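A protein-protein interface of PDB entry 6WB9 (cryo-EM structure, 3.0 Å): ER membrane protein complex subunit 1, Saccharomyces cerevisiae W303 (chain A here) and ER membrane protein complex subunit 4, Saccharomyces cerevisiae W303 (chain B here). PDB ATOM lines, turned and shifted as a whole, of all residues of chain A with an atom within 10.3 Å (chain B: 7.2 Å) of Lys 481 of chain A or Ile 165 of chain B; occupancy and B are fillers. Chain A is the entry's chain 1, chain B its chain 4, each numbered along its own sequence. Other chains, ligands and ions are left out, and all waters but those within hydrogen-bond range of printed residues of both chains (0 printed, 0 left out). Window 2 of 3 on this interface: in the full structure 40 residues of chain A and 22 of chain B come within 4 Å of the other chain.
The backbone carbonyl oxygen (O) of Lys 481 of chain A is in hydrogen-bond range of the backbone NH (N) of Gly 170 of chain B (2.7 Å).
N of Asp 569 of chain A is in hydrogen-bond range of O of Val 483 of chain A (2.7 Å). OD1 of Asn 167 of chain B sits close to O of Ile 165 of chain B, 3.0 Å away.
Gly 170 of chain B touches Thr 477 of chain A. Lys 481 of chain A touches Gly 163 of chain B. O of Ile 165 of chain B touches CE of Lys 481 of chain A, at 3.9 Å. Lys 481 of chain A touches Ala 168 of chain B (O to CB, 3.3 Å). Lys 481 of chain A touches Lys 169 of chain B (O to N, 3.6 Å). OD2 of Asp 171 of chain B touches CE of Lys 481 of chain A (3.3 Å). CG2 of Val 483 of chain A touches O of Lys 169 of chain B, 3.4 Å away. CG2 of Val 483 of chain A touches CA of Gly 170 of chain B, at 3.7 Å. OH of Tyr 485 of chain A touches CE of Lys 169 of chain B (3.3 Å). Asp 569 of chain A touches Lys 169 of chain B.
Lys 481 of chain A touches just these residues of chain B: Gly 163 (3.3 Å), Ile 165 (3.9 Å), Ala 168 (3.3 Å), Lys 169 (3.6 Å), Gly 170 (2.7 Å) and Asp 171 (3.3 Å). Printed residues of chain B within 4 Å of Val 483 of chain A: Lys 169 and Gly 170. Printed residues of chain B within 4 Å of Tyr 485 of chain A: Lys 169. Phe 656 of chain A touches none of the printed residues of chain B. No residue of chain A comes within 4 Å of Tyr 156 of chain B. Leu 159 of chain B touches none of the printed residues of chain A. No residue of chain A comes within 4 Å of Asn 160 of chain B. Gly 163 of chain B touches just one residue of chain A: Lys 481. No residue of chain A comes within 4 Å of Leu 164 of chain B. Ile 165 of chain B touches just one residue of chain A: Lys 481 (3.9 Å). No residue of chain A comes within 4 Å of Pro 166 of chain B. No residue of chain A comes within 4 Å of Asn 167 of chain B. Printed residues of chain A within 4 Å of Lys 169 of chain B: Lys 481 (3.6 Å), Val 483 (3.4 Å), Tyr 485 (3.3 Å) and Asp 569 (3.3 Å). Gly 170 of chain B touches just these residues of chain A: Thr 477, Lys 481 and Val 483. The nearest residue of chain B that does not touch Lys 481 of chain A is Asn 167 of chain B (4.8 Å).
Of the 19 printed residues of chain A, 5 touch a printed residue of chain B. Printed residues of chain A that touch a printed residue of chain B: Thr 477, Lys 481, Val 483, Tyr 485 and Asp 569. Hydrophobic or aromatic side chains of chain A that line the printed part of chain B: Val 483 and Tyr 485. Of the 19 printed residues of chain B, 6 touch a printed residue of chain A. Printed residues of chain B that touch a printed residue of chain A: Gly 163, Ile 165, Ala 168, Lys 169, Gly 170 and Asp 171. Hydrophobic or aromatic side chains of chain B that line the printed part of chain A: Ala 168. Among the printed residues, 11 pairs touch across the chains. Among the printed residues, no Asp or Glu carboxylate lies within 4 Å of a Lys or Arg side-chain nitrogen of the other chain.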
ATOM      1  N   GLY A 475      20.678 -31.797  29.144  1.00  0.00           N
ATOM      2  CA  GLY A 475      19.720 -31.142  29.999  1.00  0.00           C
ATOM      3  C   GLY A 475      18.304 -31.459  29.583  1.00  0.00           C
ATOM      4  O   GLY A 475      18.066 -32.282  28.698  1.00  0.00           O
ATOM      5  N   ILE A 476      17.359 -30.790  30.236  1.00  0.00           N
ATOM      6  CA  ILE A 476      15.933 -30.988  30.004  1.00  0.00           C
ATOM      7  C   ILE A 476      15.392 -29.759  29.288  1.00  0.00           C
ATOM      8  O   ILE A 476      15.464 -28.642  29.814  1.00  0.00           O
ATOM      9  CB  ILE A 476      15.170 -31.245  31.315  1.00  0.00           C
ATOM     10  CG1 ILE A 476      15.456 -32.649  31.843  1.00  0.00           C
ATOM     11  CG2 ILE A 476      13.679 -31.086  31.114  1.00  0.00           C
ATOM     12  CD1 ILE A 476      16.512 -32.700  32.899  1.00  0.00           C
ATOM     13  N   THR A 477      14.859 -29.960  28.084  1.00  0.00           N
ATOM     14  CA  THR A 477      14.239 -28.877  27.331  1.00  0.00           C
ATOM     15  C   THR A 477      12.819 -28.656  27.835  1.00  0.00           C
ATOM     16  O   THR A 477      12.004 -29.582  27.836  1.00  0.00           O
ATOM     17  CB  THR A 477      14.223 -29.193  25.837  1.00  0.00           C
ATOM     18  OG1 THR A 477      13.509 -30.414  25.614  1.00  0.00           O
ATOM     19  CG2 THR A 477      15.628 -29.342  25.315  1.00  0.00           C
ATOM     20  N   LEU A 478      12.525 -27.432  28.255  1.00  0.00           N
ATOM     21  CA  LEU A 478      11.207 -27.084  28.758  1.00  0.00           C
ATOM     22  C   LEU A 478      10.298 -26.706  27.587  1.00  0.00           C
ATOM     23  O   LEU A 478      10.635 -26.910  26.419  1.00  0.00           O
ATOM     24  CB  LEU A 478      11.326 -25.967  29.791  1.00  0.00           C
ATOM     25  CG  LEU A 478      12.202 -26.277  31.007  1.00  0.00           C
ATOM     26  CD1 LEU A 478      12.214 -25.112  31.975  1.00  0.00           C
ATOM     27  CD2 LEU A 478      11.750 -27.547  31.700  1.00  0.00           C
ATOM     28  N   GLY A 479       9.122 -26.154  27.893  1.00  0.00           N
ATOM     29  CA  GLY A 479       8.204 -25.758  26.840  1.00  0.00           C
ATOM     30  C   GLY A 479       8.642 -24.513  26.099  1.00  0.00           C
ATOM     31  O   GLY A 479       8.271 -24.313  24.938  1.00  0.00           O
ATOM     32  N   ASP A 480       9.436 -23.666  26.746  1.00  0.00           N
ATOM     33  CA  ASP A 480       9.999 -22.480  26.121  1.00  0.00           C
ATOM     34  C   ASP A 480      11.319 -22.761  25.418  1.00  0.00           C
ATOM     35  O   ASP A 480      12.030 -21.809  25.074  1.00  0.00           O
ATOM     36  CB  ASP A 480      10.194 -21.382  27.166  1.00  0.00           C
ATOM     37  CG  ASP A 480       8.900 -20.996  27.851  1.00  0.00           C
ATOM     38  OD1 ASP A 480       7.857 -20.935  27.166  1.00  0.00           O
ATOM     39  OD2 ASP A 480       8.923 -20.755  29.076  1.00  0.00           O
ATOM     40  N   LYS A 481      11.649 -24.044  25.209  1.00  0.00           N
ATOM     41  CA  LYS A 481      12.930 -24.515  24.663  1.00  0.00           C
ATOM     42  C   LYS A 481      14.117 -23.994  25.468  1.00  0.00           C
ATOM     43  O   LYS A 481      15.186 -23.725  24.922  1.00  0.00           O
ATOM     44  CB  LYS A 481      13.078 -24.165  23.180  1.00  0.00           C
ATOM     45  CG  LYS A 481      12.001 -24.764  22.295  1.00  0.00           C
ATOM     46  CD  LYS A 481      12.272 -24.486  20.828  1.00  0.00           C
ATOM     47  CE  LYS A 481      12.346 -22.996  20.548  1.00  0.00           C
ATOM     48  NZ  LYS A 481      11.095 -22.295  20.941  1.00  0.00           N
ATOM     49  N   SER A 482      13.937 -23.851  26.777  1.00  0.00           N
ATOM     50  CA  SER A 482      14.978 -23.365  27.671  1.00  0.00           C
ATOM     51  C   SER A 482      15.481 -24.552  28.481  1.00  0.00           C
ATOM     52  O   SER A 482      14.697 -25.241  29.136  1.00  0.00           O
ATOM     53  CB  SER A 482      14.445 -22.253  28.568  1.00  0.00           C
ATOM     54  OG  SER A 482      13.270 -22.660  29.241  1.00  0.00           O
ATOM     55  N   VAL A 483      16.782 -24.793  28.429  1.00  0.00           N
ATOM     56  CA  VAL A 483      17.354 -26.011  28.985  1.00  0.00           C
ATOM     57  C   VAL A 483      17.556 -25.849  30.485  1.00  0.00           C
ATOM     58  O   VAL A 483      18.129 -24.854  30.943  1.00  0.00           O
ATOM     59  CB  VAL A 483      18.678 -26.348  28.286  1.00  0.00           C
ATOM     60  CG1 VAL A 483      19.266 -27.619  28.842  1.00  0.00           C
ATOM     61  CG2 VAL A 483      18.459 -26.485  26.808  1.00  0.00           C
ATOM     62  N   LEU A 484      17.071 -26.822  31.252  1.00  0.00           N
ATOM     63  CA  LEU A 484      17.524 -27.043  32.620  1.00  0.00           C
ATOM     64  C   LEU A 484      18.612 -28.105  32.566  1.00  0.00           C
ATOM     65  O   LEU A 484      18.328 -29.280  32.323  1.00  0.00           O
ATOM     66  CB  LEU A 484      16.375 -27.485  33.520  1.00  0.00           C
ATOM     67  CG  LEU A 484      15.616 -26.377  34.236  1.00  0.00           C
ATOM     68  CD1 LEU A 484      14.548 -26.973  35.105  1.00  0.00           C
ATOM     69  CD2 LEU A 484      16.566 -25.559  35.068  1.00  0.00           C
ATOM     70  N   TYR A 485      19.853 -27.696  32.791  1.00  0.00           N
ATOM     71  CA  TYR A 485      20.985 -28.588  32.599  1.00  0.00           C
ATOM     72  C   TYR A 485      21.117 -29.532  33.782  1.00  0.00           C
ATOM     73  O   TYR A 485      21.045 -29.105  34.936  1.00  0.00           O
ATOM     74  CB  TYR A 485      22.266 -27.782  32.411  1.00  0.00           C
ATOM     75  CG  TYR A 485      22.320 -27.050  31.095  1.00  0.00           C
ATOM     76  CD1 TYR A 485      22.876 -27.647  29.975  1.00  0.00           C
ATOM     77  CD2 TYR A 485      21.804 -25.768  30.968  1.00  0.00           C
ATOM     78  CE1 TYR A 485      22.924 -26.987  28.771  1.00  0.00           C
ATOM     79  CE2 TYR A 485      21.846 -25.100  29.768  1.00  0.00           C
ATOM     80  CZ  TYR A 485      22.409 -25.715  28.674  1.00  0.00           C
ATOM     81  OH  TYR A 485      22.457 -25.058  27.470  1.00  0.00           O
ATOM     82  N   PRO A 568      16.502 -21.680  34.088  1.00  0.00           N
ATOM     83  CA  PRO A 568      16.807 -22.305  32.797  1.00  0.00           C
ATOM     84  C   PRO A 568      17.804 -21.488  31.990  1.00  0.00           C
ATOM     85  O   PRO A 568      17.964 -20.282  32.191  1.00  0.00           O
ATOM     86  CB  PRO A 568      15.442 -22.360  32.103  1.00  0.00           C
ATOM     87  CG  PRO A 568      14.449 -22.260  33.205  1.00  0.00           C
ATOM     88  CD  PRO A 568      15.074 -21.349  34.206  1.00  0.00           C
ATOM     89  N   ASP A 569      18.485 -22.194  31.073  1.00  0.00           N
ATOM     90  CA  ASP A 569      19.539 -21.652  30.204  1.00  0.00           C
ATOM     91  C   ASP A 569      20.680 -21.035  31.010  1.00  0.00           C
ATOM     92  O   ASP A 569      21.204 -19.975  30.668  1.00  0.00           O
ATOM     93  CB  ASP A 569      18.981 -20.643  29.195  1.00  0.00           C
ATOM     94  CG  ASP A 569      18.058 -21.282  28.184  1.00  0.00           C
ATOM     95  OD1 ASP A 569      18.228 -22.485  27.906  1.00  0.00           O
ATOM     96  OD2 ASP A 569      17.170 -20.580  27.658  1.00  0.00           O
ATOM     97  N   GLU A 570      21.068 -21.706  32.090  1.00  0.00           N
ATOM     98  CA  GLU A 570      22.063 -21.215  33.039  1.00  0.00           C
ATOM     99  C   GLU A 570      23.060 -22.320  33.375  1.00  0.00           C
ATOM    100  O   GLU A 570      23.220 -22.719  34.530  1.00  0.00           O
ATOM    101  CB  GLU A 570      21.388 -20.651  34.287  1.00  0.00           C
ATOM    102  CG  GLU A 570      22.249 -19.706  35.125  1.00  0.00           C
ATOM    103  CD  GLU A 570      22.658 -18.457  34.372  1.00  0.00           C
ATOM    104  OE1 GLU A 570      21.796 -17.858  33.696  1.00  0.00           O
ATOM    105  OE2 GLU A 570      23.845 -18.077  34.456  1.00  0.00           O
ATOM    106  N   LYS A 652       2.786 -22.580  31.375  1.00  0.00           N
ATOM    107  CA  LYS A 652       3.525 -23.322  30.357  1.00  0.00           C
ATOM    108  C   LYS A 652       5.013 -23.042  30.548  1.00  0.00           C
ATOM    109  O   LYS A 652       5.608 -22.196  29.880  1.00  0.00           O
ATOM    110  CB  LYS A 652       3.058 -22.953  28.950  1.00  0.00           C
ATOM    111  CG  LYS A 652       3.525 -23.935  27.886  1.00  0.00           C
ATOM    112  CD  LYS A 652       2.946 -25.320  28.139  1.00  0.00           C
ATOM    113  CE  LYS A 652       3.517 -26.355  27.183  1.00  0.00           C
ATOM    114  NZ  LYS A 652       4.945 -26.648  27.467  1.00  0.00           N
ATOM    115  N   LYS A 653       5.612 -23.779  31.479  1.00  0.00           N
ATOM    116  CA  LYS A 653       7.054 -23.879  31.611  1.00  0.00           C
ATOM    117  C   LYS A 653       7.488 -25.331  31.714  1.00  0.00           C
ATOM    118  O   LYS A 653       8.688 -25.603  31.819  1.00  0.00           O
ATOM    119  CB  LYS A 653       7.555 -23.106  32.843  1.00  0.00           C
ATOM    120  CG  LYS A 653       7.251 -21.614  32.833  1.00  0.00           C
ATOM    121  CD  LYS A 653       7.825 -20.928  34.061  1.00  0.00           C
ATOM    122  CE  LYS A 653       7.327 -19.496  34.179  1.00  0.00           C
ATOM    123  NZ  LYS A 653       5.850 -19.439  34.362  1.00  0.00           N
ATOM    124  N   LYS A 654       6.541 -26.264  31.698  1.00  0.00           N
ATOM    125  CA  LYS A 654       6.815 -27.686  31.740  1.00  0.00           C
ATOM    126  C   LYS A 654       7.254 -28.180  30.367  1.00  0.00           C
ATOM    127  O   LYS A 654       7.072 -27.510  29.351  1.00  0.00           O
ATOM    128  CB  LYS A 654       5.573 -28.452  32.189  1.00  0.00           C
ATOM    129  CG  LYS A 654       4.380 -28.241  31.274  1.00  0.00           C
ATOM    130  CD  LYS A 654       3.232 -29.168  31.622  1.00  0.00           C
ATOM    131  CE  LYS A 654       2.052 -28.944  30.699  1.00  0.00           C
ATOM    132  NZ  LYS A 654       1.542 -27.551  30.808  1.00  0.00           N
ATOM    133  N   GLU A 655       7.822 -29.380  30.348  1.00  0.00           N
ATOM    134  CA  GLU A 655       8.327 -29.972  29.118  1.00  0.00           C
ATOM    135  C   GLU A 655       7.178 -30.600  28.330  1.00  0.00           C
ATOM    136  O   GLU A 655       5.999 -30.438  28.658  1.00  0.00           O
ATOM    137  CB  GLU A 655       9.424 -30.981  29.439  1.00  0.00           C
ATOM    138  CG  GLU A 655       8.956 -32.164  30.265  1.00  0.00           C
ATOM    139  CD  GLU A 655      10.093 -33.074  30.662  1.00  0.00           C
ATOM    140  OE1 GLU A 655      11.167 -32.988  30.029  1.00  0.00           O
ATOM    141  OE2 GLU A 655       9.917 -33.872  31.606  1.00  0.00           O
ATOM    142  N   PHE A 656       7.511 -31.332  27.270  1.00  0.00           N
ATOM    143  CA  PHE A 656       6.501 -31.962  26.430  1.00  0.00           C
ATOM    144  C   PHE A 656       5.947 -33.194  27.130  1.00  0.00           C
ATOM    145  O   PHE A 656       6.698 -34.135  27.417  1.00  0.00           O
ATOM    146  CB  PHE A 656       7.088 -32.336  25.073  1.00  0.00           C
ATOM    147  CG  PHE A 656       6.196 -33.221  24.252  1.00  0.00           C
ATOM    148  CD1 PHE A 656       4.959 -32.769  23.817  1.00  0.00           C
ATOM    149  CD2 PHE A 656       6.599 -34.501  23.903  1.00  0.00           C
ATOM    150  CE1 PHE A 656       4.138 -33.580  23.056  1.00  0.00           C
ATOM    151  CE2 PHE A 656       5.782 -35.319  23.143  1.00  0.00           C
ATOM    152  CZ  PHE A 656       4.550 -34.857  22.720  1.00  0.00           C
ATOM    153  N   LEU B 110       5.415 -18.365   4.195  1.00  0.00           N
ATOM    154  CA  LEU B 110       6.799 -17.912   4.126  1.00  0.00           C
ATOM    155  C   LEU B 110       7.271 -17.777   2.681  1.00  0.00           C
ATOM    156  O   LEU B 110       7.858 -16.758   2.305  1.00  0.00           O
ATOM    157  CB  LEU B 110       7.705 -18.876   4.895  1.00  0.00           C
ATOM    158  CG  LEU B 110       7.503 -18.982   6.406  1.00  0.00           C
ATOM    159  CD1 LEU B 110       8.375 -20.082   6.990  1.00  0.00           C
ATOM    160  CD2 LEU B 110       7.789 -17.654   7.081  1.00  0.00           C
ATOM    161  N   GLY B 155       3.459 -15.460   9.075  1.00  0.00           N
ATOM    162  CA  GLY B 155       3.869 -16.859   9.070  1.00  0.00           C
ATOM    163  C   GLY B 155       5.080 -17.127   9.948  1.00  0.00           C
ATOM    164  O   GLY B 155       5.178 -18.184  10.582  1.00  0.00           O
ATOM    165  N   TYR B 156       6.011 -16.168  10.007  1.00  0.00           N
ATOM    166  CA  TYR B 156       7.158 -16.278  10.905  1.00  0.00           C
ATOM    167  C   TYR B 156       6.725 -16.243  12.364  1.00  0.00           C
ATOM    168  O   TYR B 156       7.279 -16.964  13.199  1.00  0.00           O
ATOM    169  CB  TYR B 156       8.150 -15.150  10.616  1.00  0.00           C
ATOM    170  CG  TYR B 156       9.408 -15.172  11.455  1.00  0.00           C
ATOM    171  CD1 TYR B 156      10.495 -15.953  11.085  1.00  0.00           C
ATOM    172  CD2 TYR B 156       9.522 -14.390  12.602  1.00  0.00           C
ATOM    173  CE1 TYR B 156      11.654 -15.967  11.839  1.00  0.00           C
ATOM    174  CE2 TYR B 156      10.672 -14.404  13.366  1.00  0.00           C
ATOM    175  CZ  TYR B 156      11.735 -15.194  12.978  1.00  0.00           C
ATOM    176  OH  TYR B 156      12.885 -15.207  13.732  1.00  0.00           O
ATOM    177  N   ARG B 157       5.740 -15.402  12.685  1.00  0.00           N
ATOM    178  CA  ARG B 157       5.190 -15.343  14.035  1.00  0.00           C
ATOM    179  C   ARG B 157       4.504 -16.651  14.403  1.00  0.00           C
ATOM    180  O   ARG B 157       4.616 -17.119  15.542  1.00  0.00           O
ATOM    181  CB  ARG B 157       4.217 -14.167  14.139  1.00  0.00           C
ATOM    182  CG  ARG B 157       3.444 -14.074  15.444  1.00  0.00           C
ATOM    183  CD  ARG B 157       4.273 -13.447  16.548  1.00  0.00           C
ATOM    184  NE  ARG B 157       4.392 -12.002  16.387  1.00  0.00           N
ATOM    185  CZ  ARG B 157       4.942 -11.194  17.286  1.00  0.00           C
ATOM    186  NH1 ARG B 157       5.428 -11.689  18.416  1.00  0.00           N
ATOM    187  NH2 ARG B 157       5.006  -9.889  17.057  1.00  0.00           N
ATOM    188  N   LYS B 158       3.825 -17.275  13.436  1.00  0.00           N
ATOM    189  CA  LYS B 158       3.200 -18.574  13.683  1.00  0.00           C
ATOM    190  C   LYS B 158       4.241 -19.663  13.927  1.00  0.00           C
ATOM    191  O   LYS B 158       4.101 -20.463  14.863  1.00  0.00           O
ATOM    192  CB  LYS B 158       2.296 -18.955  12.512  1.00  0.00           C
ATOM    193  CG  LYS B 158       1.531 -20.250  12.724  1.00  0.00           C
ATOM    194  CD  LYS B 158       0.678 -20.179  13.978  1.00  0.00           C
ATOM    195  CE  LYS B 158      -0.090 -21.465  14.196  1.00  0.00           C
ATOM    196  NZ  LYS B 158      -0.920 -21.406  15.428  1.00  0.00           N
ATOM    197  N   LEU B 159       5.295 -19.701  13.102  1.00  0.00           N
ATOM    198  CA  LEU B 159       6.351 -20.697  13.283  1.00  0.00           C
ATOM    199  C   LEU B 159       7.128 -20.470  14.576  1.00  0.00           C
ATOM    200  O   LEU B 159       7.587 -21.431  15.202  1.00  0.00           O
ATOM    201  CB  LEU B 159       7.303 -20.689  12.089  1.00  0.00           C
ATOM    202  CG  LEU B 159       6.822 -21.361  10.803  1.00  0.00           C
ATOM    203  CD1 LEU B 159       7.947 -21.408   9.788  1.00  0.00           C
ATOM    204  CD2 LEU B 159       6.294 -22.757  11.083  1.00  0.00           C
ATOM    205  N   ASN B 160       7.286 -19.215  14.995  1.00  0.00           N
ATOM    206  CA  ASN B 160       7.997 -18.932  16.235  1.00  0.00           C
ATOM    207  C   ASN B 160       7.142 -19.220  17.460  1.00  0.00           C
ATOM    208  O   ASN B 160       7.675 -19.635  18.493  1.00  0.00           O
ATOM    209  CB  ASN B 160       8.467 -17.477  16.247  1.00  0.00           C
ATOM    210  CG  ASN B 160       9.494 -17.207  17.323  1.00  0.00           C
ATOM    211  OD1 ASN B 160      10.132 -18.127  17.829  1.00  0.00           O
ATOM    212  ND2 ASN B 160       9.662 -15.940  17.676  1.00  0.00           N
ATOM    213  N   SER B 161       5.827 -19.009  17.374  1.00  0.00           N
ATOM    214  CA  SER B 161       4.946 -19.385  18.470  1.00  0.00           C
ATOM    215  C   SER B 161       4.737 -20.888  18.551  1.00  0.00           C
ATOM    216  O   SER B 161       4.375 -21.393  19.619  1.00  0.00           O
ATOM    217  CB  SER B 161       3.596 -18.678  18.336  1.00  0.00           C
ATOM    218  OG  SER B 161       3.718 -17.296  18.626  1.00  0.00           O
ATOM    219  N   MET B 162       4.952 -21.614  17.450  1.00  0.00           N
ATOM    220  CA  MET B 162       4.999 -23.068  17.541  1.00  0.00           C
ATOM    221  C   MET B 162       6.262 -23.545  18.241  1.00  0.00           C
ATOM    222  O   MET B 162       6.268 -24.631  18.831  1.00  0.00           O
ATOM    223  CB  MET B 162       4.915 -23.693  16.153  1.00  0.00           C
ATOM    224  CG  MET B 162       3.528 -23.725  15.573  1.00  0.00           C
ATOM    225  SD  MET B 162       3.487 -24.647  14.034  1.00  0.00           S
ATOM    226  CE  MET B 162       1.723 -24.759  13.793  1.00  0.00           C
ATOM    227  N   GLY B 163       7.330 -22.758  18.191  1.00  0.00           N
ATOM    228  CA  GLY B 163       8.618 -23.190  18.682  1.00  0.00           C
ATOM    229  C   GLY B 163       9.467 -23.894  17.653  1.00  0.00           C
ATOM    230  O   GLY B 163      10.463 -24.527  18.022  1.00  0.00           O
ATOM    231  N   LEU B 164       9.109 -23.799  16.377  1.00  0.00           N
ATOM    232  CA  LEU B 164       9.767 -24.527  15.303  1.00  0.00           C
ATOM    233  C   LEU B 164      10.943 -23.767  14.703  1.00  0.00           C
ATOM    234  O   LEU B 164      11.447 -24.167  13.651  1.00  0.00           O
ATOM    235  CB  LEU B 164       8.752 -24.861  14.209  1.00  0.00           C
ATOM    236  CG  LEU B 164       8.795 -26.273  13.633  1.00  0.00           C
ATOM    237  CD1 LEU B 164       8.640 -27.302  14.736  1.00  0.00           C
ATOM    238  CD2 LEU B 164       7.709 -26.444  12.591  1.00  0.00           C
ATOM    239  N   ILE B 165      11.389 -22.690  15.337  1.00  0.00           N
ATOM    240  CA  ILE B 165      12.498 -21.882  14.850  1.00  0.00           C
ATOM    241  C   ILE B 165      13.635 -21.980  15.861  1.00  0.00           C
ATOM    242  O   ILE B 165      13.430 -21.703  17.046  1.00  0.00           O
ATOM    243  CB  ILE B 165      12.089 -20.418  14.625  1.00  0.00           C
ATOM    244  CG1 ILE B 165      10.937 -20.353  13.626  1.00  0.00           C
ATOM    245  CG2 ILE B 165      13.270 -19.603  14.127  1.00  0.00           C
ATOM    246  CD1 ILE B 165      10.424 -18.971  13.378  1.00  0.00           C
ATOM    247  N   PRO B 166      14.847 -22.373  15.446  1.00  0.00           N
ATOM    248  CA  PRO B 166      15.936 -22.590  16.410  1.00  0.00           C
ATOM    249  C   PRO B 166      16.493 -21.310  17.012  1.00  0.00           C
ATOM    250  O   PRO B 166      17.569 -20.849  16.622  1.00  0.00           O
ATOM    251  CB  PRO B 166      17.002 -23.312  15.575  1.00  0.00           C
ATOM    252  CG  PRO B 166      16.293 -23.806  14.360  1.00  0.00           C
ATOM    253  CD  PRO B 166      15.217 -22.815  14.094  1.00  0.00           C
ATOM    254  N   ASN B 167      15.768 -20.730  17.966  1.00  0.00           N
ATOM    255  CA  ASN B 167      16.219 -19.523  18.649  1.00  0.00           C
ATOM    256  C   ASN B 167      16.919 -19.851  19.966  1.00  0.00           C
ATOM    257  O   ASN B 167      18.082 -19.488  20.168  1.00  0.00           O
ATOM    258  CB  ASN B 167      15.035 -18.585  18.905  1.00  0.00           C
ATOM    259  CG  ASN B 167      14.187 -18.369  17.676  1.00  0.00           C
ATOM    260  OD1 ASN B 167      13.023 -18.762  17.636  1.00  0.00           O
ATOM    261  ND2 ASN B 167      14.764 -17.735  16.662  1.00  0.00           N
ATOM    262  N   ALA B 168      16.220 -20.538  20.865  1.00  0.00           N
ATOM    263  CA  ALA B 168      16.697 -20.749  22.222  1.00  0.00           C
ATOM    264  C   ALA B 168      17.668 -21.925  22.281  1.00  0.00           C
ATOM    265  O   ALA B 168      18.024 -22.531  21.266  1.00  0.00           O
ATOM    266  CB  ALA B 168      15.517 -20.956  23.165  1.00  0.00           C
ATOM    267  N   LYS B 169      18.101 -22.257  23.499  1.00  0.00           N
ATOM    268  CA  LYS B 169      19.138 -23.260  23.703  1.00  0.00           C
ATOM    269  C   LYS B 169      18.615 -24.689  23.664  1.00  0.00           C
ATOM    270  O   LYS B 169      19.425 -25.621  23.653  1.00  0.00           O
ATOM    271  CB  LYS B 169      19.847 -23.020  25.035  1.00  0.00           C
ATOM    272  CG  LYS B 169      20.267 -21.582  25.254  1.00  0.00           C
ATOM    273  CD  LYS B 169      21.269 -21.463  26.383  1.00  0.00           C
ATOM    274  CE  LYS B 169      22.589 -22.104  26.009  1.00  0.00           C
ATOM    275  NZ  LYS B 169      23.147 -21.535  24.753  1.00  0.00           N
ATOM    276  N   GLY B 170      17.300 -24.889  23.644  1.00  0.00           N
ATOM    277  CA  GLY B 170      16.761 -26.230  23.536  1.00  0.00           C
ATOM    278  C   GLY B 170      16.888 -26.859  22.172  1.00  0.00           C
ATOM    279  O   GLY B 170      16.711 -28.074  22.043  1.00  0.00           O
ATOM    280  N   ASP B 171      17.181 -26.057  21.152  1.00  0.00           N
ATOM    281  CA  ASP B 171      17.411 -26.565  19.809  1.00  0.00           C
ATOM    282  C   ASP B 171      18.869 -26.915  19.570  1.00  0.00           C
ATOM    283  O   ASP B 171      19.158 -27.866  18.836  1.00  0.00           O
ATOM    284  CB  ASP B 171      16.951 -25.534  18.779  1.00  0.00           C
ATOM    285  CG  ASP B 171      15.525 -25.084  19.009  1.00  0.00           C
ATOM    286  OD1 ASP B 171      14.599 -25.896  18.812  1.00  0.00           O
ATOM    287  OD2 ASP B 171      15.328 -23.921  19.413  1.00  0.00           O
ATOM    288  N   TRP B 172      19.791 -26.171  20.179  1.00  0.00           N
ATOM    289  CA  TRP B 172      21.220 -26.405  20.031  1.00  0.00           C
ATOM    290  C   TRP B 172      21.810 -27.146  21.220  1.00  0.00           C
ATOM    291  O   TRP B 172      23.024 -27.097  21.436  1.00  0.00           O
ATOM    292  CB  TRP B 172      21.947 -25.078  19.811  1.00  0.00           C
ATOM    293  CG  TRP B 172      21.371 -24.275  18.682  1.00  0.00           C
ATOM    294  CD1 TRP B 172      20.714 -23.087  18.778  1.00  0.00           C
ATOM    295  CD2 TRP B 172      21.385 -24.616  17.290  1.00  0.00           C
ATOM    296  NE1 TRP B 172      20.325 -22.660  17.533  1.00  0.00           N
ATOM    297  CE2 TRP B 172      20.724 -23.583  16.603  1.00  0.00           C
ATOM    298  CE3 TRP B 172      21.896 -25.693  16.558  1.00  0.00           C
ATOM    299  CZ2 TRP B 172      20.565 -23.592  15.220  1.00  0.00           C
ATOM    300  CZ3 TRP B 172      21.731 -25.703  15.189  1.00  0.00           C
ATOM    301  CH2 TRP B 172      21.071 -24.660  14.533  1.00  0.00           C
